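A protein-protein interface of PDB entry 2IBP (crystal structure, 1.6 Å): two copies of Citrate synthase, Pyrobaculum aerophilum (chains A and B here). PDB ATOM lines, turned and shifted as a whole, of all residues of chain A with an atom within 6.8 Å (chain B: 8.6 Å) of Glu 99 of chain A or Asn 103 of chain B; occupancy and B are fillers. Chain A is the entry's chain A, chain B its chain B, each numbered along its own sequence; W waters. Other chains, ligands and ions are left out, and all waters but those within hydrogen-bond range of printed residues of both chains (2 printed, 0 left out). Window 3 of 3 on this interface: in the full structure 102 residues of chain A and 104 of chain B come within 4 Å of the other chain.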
ATOM      1  N   HIS A  94     -16.550  -5.990 -18.859  1.00  0.00           N
ATOM      2  CA  HIS A  94     -17.068  -6.968 -17.913  1.00  0.00           C
ATOM      3  C   HIS A  94     -15.997  -7.210 -16.845  1.00  0.00           C
ATOM      4  O   HIS A  94     -14.790  -7.213 -17.147  1.00  0.00           O
ATOM      5  CB  HIS A  94     -17.347  -8.276 -18.657  1.00  0.00           C
ATOM      6  CG  HIS A  94     -18.069  -9.303 -17.840  1.00  0.00           C
ATOM      7  ND1 HIS A  94     -17.441 -10.078 -16.887  1.00  0.00           N
ATOM      8  CD2 HIS A  94     -19.362  -9.712 -17.865  1.00  0.00           C
ATOM      9  CE1 HIS A  94     -18.325 -10.891 -16.333  1.00  0.00           C
ATOM     10  NE2 HIS A  94     -19.500 -10.688 -16.907  1.00  0.00           N
ATOM     11  N   PRO A  95     -16.401  -7.385 -15.583  1.00  0.00           N
ATOM     12  CA  PRO A  95     -15.388  -7.610 -14.564  1.00  0.00           C
ATOM     13  C   PRO A  95     -14.392  -8.734 -14.885  1.00  0.00           C
ATOM     14  O   PRO A  95     -13.224  -8.627 -14.541  1.00  0.00           O
ATOM     15  CB  PRO A  95     -16.219  -7.932 -13.315  1.00  0.00           C
ATOM     16  CG  PRO A  95     -17.490  -7.219 -13.527  1.00  0.00           C
ATOM     17  CD  PRO A  95     -17.753  -7.286 -15.002  1.00  0.00           C
ATOM     18  N   ALA A  96     -14.845  -9.805 -15.537  1.00  0.00           N
ATOM     19  CA  ALA A  96     -13.960 -10.916 -15.878  1.00  0.00           C
ATOM     20  C   ALA A  96     -12.877 -10.444 -16.831  1.00  0.00           C
ATOM     21  O   ALA A  96     -11.712 -10.833 -16.717  1.00  0.00           O
ATOM     22  CB  ALA A  96     -14.738 -12.068 -16.502  1.00  0.00           C
ATOM     23  N   THR A  97     -13.263  -9.571 -17.755  1.00  0.00           N
ATOM     24  CA  THR A  97     -12.321  -9.009 -18.720  1.00  0.00           C
ATOM     25  C   THR A  97     -11.259  -8.175 -18.001  1.00  0.00           C
ATOM     26  O   THR A  97     -10.077  -8.291 -18.283  1.00  0.00           O
ATOM     27  CB  THR A  97     -13.062  -8.132 -19.724  1.00  0.00           C
ATOM     28  OG1 THR A  97     -14.095  -8.914 -20.338  1.00  0.00           O
ATOM     29  CG2 THR A  97     -12.117  -7.566 -20.778  1.00  0.00           C
ATOM     30  N   VAL A  98     -11.686  -7.366 -17.042  1.00  0.00           N
ATOM     31  CA  VAL A  98     -10.767  -6.534 -16.273  1.00  0.00           C
ATOM     32  C   VAL A  98      -9.783  -7.410 -15.501  1.00  0.00           C
ATOM     33  O   VAL A  98      -8.582  -7.125 -15.485  1.00  0.00           O
ATOM     34  CB  VAL A  98     -11.530  -5.592 -15.325  1.00  0.00           C
ATOM     35  CG1 VAL A  98     -10.552  -4.772 -14.492  1.00  0.00           C
ATOM     36  CG2 VAL A  98     -12.429  -4.691 -16.140  1.00  0.00           C
ATOM     37  N   GLU A  99     -10.261  -8.535 -14.966  1.00  0.00           N
ATOM     38  CA  GLU A  99      -9.356  -9.446 -14.262  1.00  0.00           C
ATOM     39  C   GLU A  99      -8.372 -10.082 -15.233  1.00  0.00           C
ATOM     40  O   GLU A  99      -7.212 -10.296 -14.888  1.00  0.00           O
ATOM     41  CB  GLU A  99     -10.117 -10.491 -13.464  1.00  0.00           C
ATOM     42  CG  GLU A  99     -10.934  -9.864 -12.343  1.00  0.00           C
ATOM     43  CD  GLU A  99     -10.092  -8.970 -11.429  1.00  0.00           C
ATOM     44  OE1 GLU A  99      -9.038  -9.437 -10.944  1.00  0.00           O
ATOM     45  OE2 GLU A  99     -10.479  -7.798 -11.204  1.00  0.00           O
ATOM     46  N   VAL A 100      -8.835 -10.427 -16.434  1.00  0.00           N
ATOM     47  CA  VAL A 100      -7.930 -10.961 -17.437  1.00  0.00           C
ATOM     48  C   VAL A 100      -6.824  -9.941 -17.728  1.00  0.00           C
ATOM     49  O   VAL A 100      -5.647 -10.272 -17.723  1.00  0.00           O
ATOM     50  CB  VAL A 100      -8.679 -11.365 -18.705  1.00  0.00           C
ATOM     51  CG1 VAL A 100      -7.719 -11.609 -19.862  1.00  0.00           C
ATOM     52  CG2 VAL A 100      -9.517 -12.605 -18.406  1.00  0.00           C
ATOM     53  N   ILE A 101      -7.204  -8.685 -17.949  1.00  0.00           N
ATOM     54  CA  ILE A 101      -6.205  -7.632 -18.182  1.00  0.00           C
ATOM     55  C   ILE A 101      -5.244  -7.492 -16.986  1.00  0.00           C
ATOM     56  O   ILE A 101      -4.028  -7.366 -17.169  1.00  0.00           O
ATOM     57  CB  ILE A 101      -6.885  -6.282 -18.474  1.00  0.00           C
ATOM     58  CG1 ILE A 101      -7.713  -6.381 -19.764  1.00  0.00           C
ATOM     59  CG2 ILE A 101      -5.827  -5.176 -18.636  1.00  0.00           C
ATOM     60  CD1 ILE A 101      -8.667  -5.175 -19.989  1.00  0.00           C
ATOM     61  N   ARG A 102      -5.780  -7.509 -15.774  1.00  0.00           N
ATOM     62  CA  ARG A 102      -4.968  -7.381 -14.560  1.00  0.00           C
ATOM     63  C   ARG A 102      -3.921  -8.481 -14.524  1.00  0.00           C
ATOM     64  O   ARG A 102      -2.742  -8.237 -14.238  1.00  0.00           O
ATOM     65  CB  ARG A 102      -5.850  -7.502 -13.322  1.00  0.00           C
ATOM     66  CG  ARG A 102      -5.108  -7.264 -12.016  1.00  0.00           C
ATOM     67  CD  ARG A 102      -5.979  -7.589 -10.819  1.00  0.00           C
ATOM     68  NE  ARG A 102      -7.265  -6.903 -10.878  1.00  0.00           N
ATOM     69  CZ  ARG A 102      -7.512  -5.693 -10.380  1.00  0.00           C
ATOM     70  NH1 ARG A 102      -6.556  -4.986  -9.792  1.00  0.00           N
ATOM     71  NH2 ARG A 102      -8.731  -5.177 -10.496  1.00  0.00           N
ATOM     72  N   ASN A 103      -4.358  -9.702 -14.810  1.00  0.00           N
ATOM     73  CA  ASN A 103      -3.426 -10.827 -14.806  1.00  0.00           C
ATOM     74  C   ASN A 103      -2.333 -10.728 -15.841  1.00  0.00           C
ATOM     75  O   ASN A 103      -1.260 -11.290 -15.653  1.00  0.00           O
ATOM     76  CB  ASN A 103      -4.145 -12.142 -14.940  1.00  0.00           C
ATOM     77  CG  ASN A 103      -4.722 -12.568 -13.642  1.00  0.00           C
ATOM     78  OD1 ASN A 103      -3.977 -12.788 -12.680  1.00  0.00           O
ATOM     79  ND2 ASN A 103      -6.039 -12.558 -13.547  1.00  0.00           N
ATOM     80  N   LEU A 104      -2.592  -9.967 -16.899  1.00  0.00           N
ATOM     81  CA  LEU A 104      -1.639  -9.768 -17.976  1.00  0.00           C
ATOM     82  C   LEU A 104      -1.009  -8.365 -17.943  1.00  0.00           C
ATOM     83  O   LEU A 104      -0.389  -7.940 -18.905  1.00  0.00           O
ATOM     84  CB  LEU A 104      -2.344 -10.019 -19.300  1.00  0.00           C
ATOM     85  CG  LEU A 104      -2.855 -11.456 -19.468  1.00  0.00           C
ATOM     86  CD1 LEU A 104      -3.498 -11.624 -20.844  1.00  0.00           C
ATOM     87  CD2 LEU A 104      -1.680 -12.396 -19.283  1.00  0.00           C
ATOM     88  N   ALA A 119     -12.021 -12.669 -23.820  1.00  0.00           N
ATOM     89  CA  ALA A 119     -12.710 -12.693 -22.533  1.00  0.00           C
ATOM     90  C   ALA A 119     -14.005 -11.911 -22.567  1.00  0.00           C
ATOM     91  O   ALA A 119     -15.018 -12.381 -22.056  1.00  0.00           O
ATOM     92  CB  ALA A 119     -11.825 -12.161 -21.423  1.00  0.00           C
ATOM     93  N   TYR A 123     -18.556 -13.536 -22.248  1.00  0.00           N
ATOM     94  CA  TYR A 123     -19.712 -13.282 -21.406  1.00  0.00           C
ATOM     95  C   TYR A 123     -20.710 -12.281 -21.993  1.00  0.00           C
ATOM     96  O   TYR A 123     -21.692 -11.929 -21.334  1.00  0.00           O
ATOM     97  CB  TYR A 123     -19.271 -12.842 -20.013  1.00  0.00           C
ATOM     98  CG  TYR A 123     -18.569 -13.930 -19.238  1.00  0.00           C
ATOM     99  CD1 TYR A 123     -19.208 -15.131 -18.970  1.00  0.00           C
ATOM    100  CD2 TYR A 123     -17.297 -13.745 -18.742  1.00  0.00           C
ATOM    101  CE1 TYR A 123     -18.575 -16.135 -18.266  1.00  0.00           C
ATOM    102  CE2 TYR A 123     -16.650 -14.741 -18.042  1.00  0.00           C
ATOM    103  CZ  TYR A 123     -17.299 -15.935 -17.797  1.00  0.00           C
ATOM    104  OH  TYR A 123     -16.673 -16.906 -17.066  1.00  0.00           O
ATOM    105  N   PHE A 168      -2.785  -0.676 -15.276  1.00  0.00           N
ATOM    106  CA  PHE A 168      -2.311  -1.813 -14.511  1.00  0.00           C
ATOM    107  C   PHE A 168      -0.821  -2.062 -14.701  1.00  0.00           C
ATOM    108  O   PHE A 168      -0.144  -2.461 -13.755  1.00  0.00           O
ATOM    109  CB  PHE A 168      -3.071  -3.093 -14.835  1.00  0.00           C
ATOM    110  CG  PHE A 168      -4.489  -3.115 -14.353  1.00  0.00           C
ATOM    111  CD1 PHE A 168      -4.814  -2.764 -13.056  1.00  0.00           C
ATOM    112  CD2 PHE A 168      -5.457  -3.723 -15.122  1.00  0.00           C
ATOM    113  CE1 PHE A 168      -6.115  -2.880 -12.593  1.00  0.00           C
ATOM    114  CE2 PHE A 168      -6.765  -3.831 -14.673  1.00  0.00           C
ATOM    115  CZ  PHE A 168      -7.080  -3.448 -13.393  1.00  0.00           C
ATOM    116  N   PRO B  95       0.767 -19.340 -13.553  1.00  0.00           N
ATOM    117  CA  PRO B  95      -0.370 -18.979 -12.703  1.00  0.00           C
ATOM    118  C   PRO B  95      -1.335 -17.962 -13.314  1.00  0.00           C
ATOM    119  O   PRO B  95      -2.539 -18.055 -13.066  1.00  0.00           O
ATOM    120  CB  PRO B  95       0.287 -18.418 -11.437  1.00  0.00           C
ATOM    121  CG  PRO B  95       1.638 -19.070 -11.406  1.00  0.00           C
ATOM    122  CD  PRO B  95       2.053 -19.222 -12.842  1.00  0.00           C
ATOM    123  N   ALA B  96      -0.834 -17.012 -14.106  1.00  0.00           N
ATOM    124  CA  ALA B  96      -1.704 -16.011 -14.746  1.00  0.00           C
ATOM    125  C   ALA B  96      -2.646 -16.704 -15.731  1.00  0.00           C
ATOM    126  O   ALA B  96      -3.809 -16.340 -15.858  1.00  0.00           O
ATOM    127  CB  ALA B  96      -0.875 -14.950 -15.464  1.00  0.00           C
ATOM    128  N   THR B  97      -2.133 -17.712 -16.420  1.00  0.00           N
ATOM    129  CA  THR B  97      -2.938 -18.462 -17.381  1.00  0.00           C
ATOM    130  C   THR B  97      -4.079 -19.179 -16.665  1.00  0.00           C
ATOM    131  O   THR B  97      -5.220 -19.163 -17.114  1.00  0.00           O
ATOM    132  CB  THR B  97      -2.081 -19.497 -18.122  1.00  0.00           C
ATOM    133  OG1 THR B  97      -0.962 -18.830 -18.721  1.00  0.00           O
ATOM    134  CG2 THR B  97      -2.903 -20.209 -19.192  1.00  0.00           C
ATOM    135  N   VAL B  98      -3.758 -19.819 -15.551  1.00  0.00           N
ATOM    136  CA  VAL B  98      -4.760 -20.533 -14.764  1.00  0.00           C
ATOM    137  C   VAL B  98      -5.821 -19.529 -14.273  1.00  0.00           C
ATOM    138  O   VAL B  98      -7.013 -19.811 -14.338  1.00  0.00           O
ATOM    139  CB  VAL B  98      -4.116 -21.279 -13.575  1.00  0.00           C
ATOM    140  CG1 VAL B  98      -5.173 -22.059 -12.813  1.00  0.00           C
ATOM    141  CG2 VAL B  98      -3.010 -22.217 -14.087  1.00  0.00           C
ATOM    142  N   GLU B  99      -5.400 -18.332 -13.877  1.00  0.00           N
ATOM    143  CA  GLU B  99      -6.381 -17.321 -13.453  1.00  0.00           C
ATOM    144  C   GLU B  99      -7.264 -16.873 -14.610  1.00  0.00           C
ATOM    145  O   GLU B  99      -8.456 -16.644 -14.429  1.00  0.00           O
ATOM    146  CB  GLU B  99      -5.718 -16.122 -12.776  1.00  0.00           C
ATOM    147  CG  GLU B  99      -5.099 -16.473 -11.455  1.00  0.00           C
ATOM    148  CD  GLU B  99      -6.063 -17.225 -10.551  1.00  0.00           C
ATOM    149  OE1 GLU B  99      -7.176 -16.718 -10.309  1.00  0.00           O
ATOM    150  OE2 GLU B  99      -5.705 -18.328 -10.080  1.00  0.00           O
ATOM    151  N   VAL B 100      -6.694 -16.763 -15.802  1.00  0.00           N
ATOM    152  CA  VAL B 100      -7.487 -16.422 -16.978  1.00  0.00           C
ATOM    153  C   VAL B 100      -8.550 -17.503 -17.193  1.00  0.00           C
ATOM    154  O   VAL B 100      -9.726 -17.196 -17.402  1.00  0.00           O
ATOM    155  CB  VAL B 100      -6.591 -16.238 -18.213  1.00  0.00           C
ATOM    156  CG1 VAL B 100      -7.407 -16.218 -19.504  1.00  0.00           C
ATOM    157  CG2 VAL B 100      -5.759 -14.965 -18.087  1.00  0.00           C
ATOM    158  N   ILE B 101      -8.140 -18.768 -17.129  1.00  0.00           N
ATOM    159  CA  ILE B 101      -9.090 -19.884 -17.274  1.00  0.00           C
ATOM    160  C   ILE B 101     -10.181 -19.822 -16.199  1.00  0.00           C
ATOM    161  O   ILE B 101     -11.369 -19.986 -16.502  1.00  0.00           O
ATOM    162  CB  ILE B 101      -8.379 -21.257 -17.237  1.00  0.00           C
ATOM    163  CG1 ILE B 101      -7.375 -21.354 -18.382  1.00  0.00           C
ATOM    164  CG2 ILE B 101      -9.408 -22.373 -17.338  1.00  0.00           C
ATOM    165  CD1 ILE B 101      -6.444 -22.526 -18.264  1.00  0.00           C
ATOM    166  N   ARG B 102      -9.782 -19.555 -14.962  1.00  0.00           N
ATOM    167  CA  ARG B 102     -10.721 -19.481 -13.858  1.00  0.00           C
ATOM    168  C   ARG B 102     -11.758 -18.393 -14.151  1.00  0.00           C
ATOM    169  O   ARG B 102     -12.960 -18.590 -13.972  1.00  0.00           O
ATOM    170  CB  ARG B 102     -10.001 -19.153 -12.563  1.00  0.00           C
ATOM    171  CG  ARG B 102     -10.877 -19.336 -11.330  1.00  0.00           C
ATOM    172  CD  ARG B 102     -10.148 -18.870 -10.073  1.00  0.00           C
ATOM    173  NE  ARG B 102      -8.806 -19.443  -9.968  1.00  0.00           N
ATOM    174  CZ  ARG B 102      -8.515 -20.610  -9.395  1.00  0.00           C
ATOM    175  NH1 ARG B 102      -9.474 -21.360  -8.858  1.00  0.00           N
ATOM    176  NH2 ARG B 102      -7.251 -21.031  -9.363  1.00  0.00           N
ATOM    177  N   ASN B 103     -11.290 -17.235 -14.596  1.00  0.00           N
ATOM    178  CA  ASN B 103     -12.212 -16.144 -14.915  1.00  0.00           C
ATOM    179  C   ASN B 103     -13.189 -16.473 -16.025  1.00  0.00           C
ATOM    180  O   ASN B 103     -14.299 -15.935 -16.071  1.00  0.00           O
ATOM    181  CB  ASN B 103     -11.461 -14.872 -15.235  1.00  0.00           C
ATOM    182  CG  ASN B 103     -11.034 -14.156 -13.992  1.00  0.00           C
ATOM    183  OD1 ASN B 103     -11.849 -13.503 -13.332  1.00  0.00           O
ATOM    184  ND2 ASN B 103      -9.767 -14.257 -13.662  1.00  0.00           N
ATOM    185  N   LEU B 104     -12.785 -17.393 -16.890  1.00  0.00           N
ATOM    186  CA  LEU B 104     -13.616 -17.825 -18.000  1.00  0.00           C
ATOM    187  C   LEU B 104     -14.239 -19.196 -17.747  1.00  0.00           C
ATOM    188  O   LEU B 104     -14.761 -19.811 -18.674  1.00  0.00           O
ATOM    189  CB  LEU B 104     -12.802 -17.835 -19.293  1.00  0.00           C
ATOM    190  CG  LEU B 104     -12.236 -16.477 -19.714  1.00  0.00           C
ATOM    191  CD1 LEU B 104     -11.419 -16.553 -21.013  1.00  0.00           C
ATOM    192  CD2 LEU B 104     -13.357 -15.460 -19.855  1.00  0.00           C
ATOM    193  N   ALA B 105     -14.309 -19.597 -16.481  1.00  0.00           N
ATOM    194  CA  ALA B 105     -14.841 -20.915 -16.131  1.00  0.00           C
ATOM    195  C   ALA B 105     -16.297 -21.097 -16.539  1.00  0.00           C
ATOM    196  O   ALA B 105     -16.715 -22.205 -16.871  1.00  0.00           O
ATOM    197  CB  ALA B 105     -14.690 -21.170 -14.644  1.00  0.00           C
ATOM    198  N   LYS B 106     -17.068 -20.016 -16.519  1.00  0.00           N
ATOM    199  CA  LYS B 106     -18.490 -20.077 -16.844  1.00  0.00           C
ATOM    200  C   LYS B 106     -18.758 -19.816 -18.321  1.00  0.00           C
ATOM    201  O   LYS B 106     -19.915 -19.782 -18.754  1.00  0.00           O
ATOM    202  CB  LYS B 106     -19.268 -19.063 -15.994  1.00  0.00           C
ATOM    203  CG  LYS B 106     -19.253 -19.338 -14.491  1.00  0.00           C
ATOM    204  CD  LYS B 106     -19.915 -18.192 -13.731  1.00  0.00           C
ATOM    205  CE  LYS B 106     -19.800 -18.370 -12.222  1.00  0.00           C
ATOM    206  NZ  LYS B 106     -20.455 -19.622 -11.752  1.00  0.00           N
ATOM    207  N   ALA B 107     -17.692 -19.578 -19.076  1.00  0.00           N
ATOM    208  CA  ALA B 107     -17.790 -19.331 -20.505  1.00  0.00           C
ATOM    209  C   ALA B 107     -17.577 -20.613 -21.295  1.00  0.00           C
ATOM    210  O   ALA B 107     -17.081 -21.627 -20.777  1.00  0.00           O
ATOM    211  CB  ALA B 107     -16.763 -18.308 -20.930  1.00  0.00           C
ATOM    212  N   ALA B 112     -12.099 -19.763 -23.535  1.00  0.00           N
ATOM    213  CA  ALA B 112     -11.065 -20.000 -22.537  1.00  0.00           C
ATOM    214  C   ALA B 112      -9.787 -20.461 -23.209  1.00  0.00           C
ATOM    215  O   ALA B 112      -8.701 -20.013 -22.828  1.00  0.00           O
ATOM    216  CB  ALA B 112     -11.512 -21.024 -21.491  1.00  0.00           C
ATOM    217  N   ALA B 115      -8.122 -17.388 -25.010  1.00  0.00           N
ATOM    218  CA  ALA B 115      -7.579 -16.450 -24.044  1.00  0.00           C
ATOM    219  C   ALA B 115      -6.397 -17.031 -23.284  1.00  0.00           C
ATOM    220  O   ALA B 115      -5.375 -16.367 -23.086  1.00  0.00           O
ATOM    221  CB  ALA B 115      -8.666 -15.999 -23.065  1.00  0.00           C
ATOM    222  N   HIS B 165     -10.152 -25.993 -17.617  1.00  0.00           N
ATOM    223  CA  HIS B 165     -11.440 -25.350 -17.862  1.00  0.00           C
ATOM    224  C   HIS B 165     -12.593 -26.282 -17.492  1.00  0.00           C
ATOM    225  O   HIS B 165     -13.553 -25.867 -16.834  1.00  0.00           O
ATOM    226  CB  HIS B 165     -11.567 -24.871 -19.288  1.00  0.00           C
ATOM    227  CG  HIS B 165     -12.791 -24.052 -19.507  1.00  0.00           C
ATOM    228  ND1 HIS B 165     -13.994 -24.610 -19.880  1.00  0.00           N
ATOM    229  CD2 HIS B 165     -13.034 -22.740 -19.279  1.00  0.00           C
ATOM    230  CE1 HIS B 165     -14.911 -23.661 -19.942  1.00  0.00           C
ATOM    231  NE2 HIS B 165     -14.349 -22.514 -19.601  1.00  0.00           N
ATOM    232  N   PHE B 168     -12.829 -26.288 -13.609  1.00  0.00           N
ATOM    233  CA  PHE B 168     -13.382 -25.047 -13.050  1.00  0.00           C
ATOM    234  C   PHE B 168     -14.848 -24.865 -13.435  1.00  0.00           C
ATOM    235  O   PHE B 168     -15.659 -24.384 -12.628  1.00  0.00           O
ATOM    236  CB  PHE B 168     -12.597 -23.819 -13.503  1.00  0.00           C
ATOM    237  CG  PHE B 168     -11.209 -23.738 -12.950  1.00  0.00           C
ATOM    238  CD1 PHE B 168     -10.972 -23.874 -11.588  1.00  0.00           C
ATOM    239  CD2 PHE B 168     -10.162 -23.343 -13.768  1.00  0.00           C
ATOM    240  CE1 PHE B 168      -9.707 -23.714 -11.072  1.00  0.00           C
ATOM    241  CE2 PHE B 168      -8.890 -23.167 -13.252  1.00  0.00           C
ATOM    242  CZ  PHE B 168      -8.659 -23.361 -11.906  1.00  0.00           C
HETATM  243  O   HOH W   1     -15.878 -17.965 -14.198  1.00  0.00           O
HETATM  244  O   HOH W   2      -8.007 -13.290 -11.526  1.00  0.00           O
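Printed residues of chain B within 4 Å of Ala 96 of chain A: Asn 103 (3.9 Å). Of chain B, only Asn 103 (3.5 Å) comes within 4 Å of Glu 99 of chain A. Of the printed residues of chain B, Asn 103 of chain A touches Ala 96 and Glu 99. Printed residues of chain B within 4 Å of Ala 119 of chain A: Leu 104 (3.9 Å). Printed residues of chain A within 4 Å of Leu 104 of chain B: Ala 119 (3.9 Å) and Tyr 123 (3.3 Å). Printed residues of chain A within 4 Å of Lys 106 of chain B: Tyr 123. The nearest residue of chain B that does not touch Glu 99 of chain A is Val 100 of chain B (5.8 Å). The nearest residue of chain A that does not touch Asn 103 of chain B is Asn 103 of chain A (4.1 Å).
Asn 103 of chain B touches Ala 96 of chain A. Glu 99 of chain A touches Asn 103 of chain B. O of Asn 103 of chain A touches CB of Ala 96 of chain B (3.7 Å). ND2 of Asn 103 of chain A touches CB of Glu 99 of chain B, at 3.7 Å. Ala 119 of chain A touches Leu 104 of chain B (CA to CD2, 3.9 Å). CA of Leu 104 of chain B touches OH of Tyr 123 of chain A, at 3.3 Å. Tyr 123 of chain A touches Ala 105 of chain B (OH to N, 3.6 Å).
Water W2 bridges the side-chain amide nitrogen of Asn 103 of chain A (2.9 Å) and the side-chain amide nitrogen of Asn 103 of chain B (2.9 Å). Water W1 lies within hydrogen-bond range of the backbone carbonyl oxygen of Arg 102 of chain B, the side-chain hydroxyl of Tyr 123 of chain A, the backbone carbonyl oxygen of Asn 103 of chain B, the backbone NH of Ala 105 of chain B and the backbone NH of Lys 106 of chain B.
Of the 14 printed residues of chain A, 5 touch a printed residue of chain B. Hydrophobic or aromatic side chains of chain A that line the printed part of chain B: Ala 96, Ala 119 and Tyr 123. Of the 17 printed residues of chain B, 7 touch a printed residue of chain A. Printed residues of chain B that touch a printed residue of chain A: Ala 96, Glu 99, Asn 103, Leu 104, Ala 105, Lys 106 and Ala 107. Hydrophobic or aromatic side chains of chain B within 4 Å of the printed part of chain A: Ala 96, Leu 104 and Ala 107.
Ala 96 of chain A touches Asn 103 of chain B, and with the chains exchanged Asn 103 of chain A touches Ala 96 of chain B. Glu 99 of chain A touches Asn 103 of chain B, and with the chains exchanged Asn 103 of chain A touches Glu 99 of chain B. Positions printed for both chains: 95, 96, 97, 98, 99, 100, 101, 102, 103, 104 and 168.
The backbone NH (N) of Lys 106 of chain B lies within hydrogen-bond range of the side-chain hydroxyl (OH) of Tyr 123 of chain A, at 3.2 Å. OH of Tyr 123 of chain A lies within hydrogen-bond range of N of Ala 107 of chain B (3.5 Å). The side-chain hydroxyl of Tyr 123 of chain A sits at hydrogen-bond distance from the backbone carbonyl oxygen of Asn 103 of chain B, at 2.8 Å.
The backbone carbonyl oxygen of Leu 104 of chain B sits at hydrogen-bond distance from a ring nitrogen (NE2) of His 165 of chain B. A ring nitrogen (ND1) of His 94 of chain A is in hydrogen-bond range of the backbone NH of Ala 96 of chain A (2.9 Å). OE1 of Glu 99 of chain B lies within salt-bridge range of NE of Arg 102 of chain B (3.2 Å). OE1 of Glu 99 of chain A lies within salt-bridge range of NE of Arg 102 of chain A (3.1 Å). A ring nitrogen (NE2) of His 165 of chain B lies close to the backbone carbonyl oxygen (O) of Ala 107 of chain B. The backbone carbonyl oxygen (O) of Glu 99 of chain B sits at hydrogen-bond distance from the side-chain amide nitrogen (ND2) of Asn 103 of chain B (2.8 Å).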
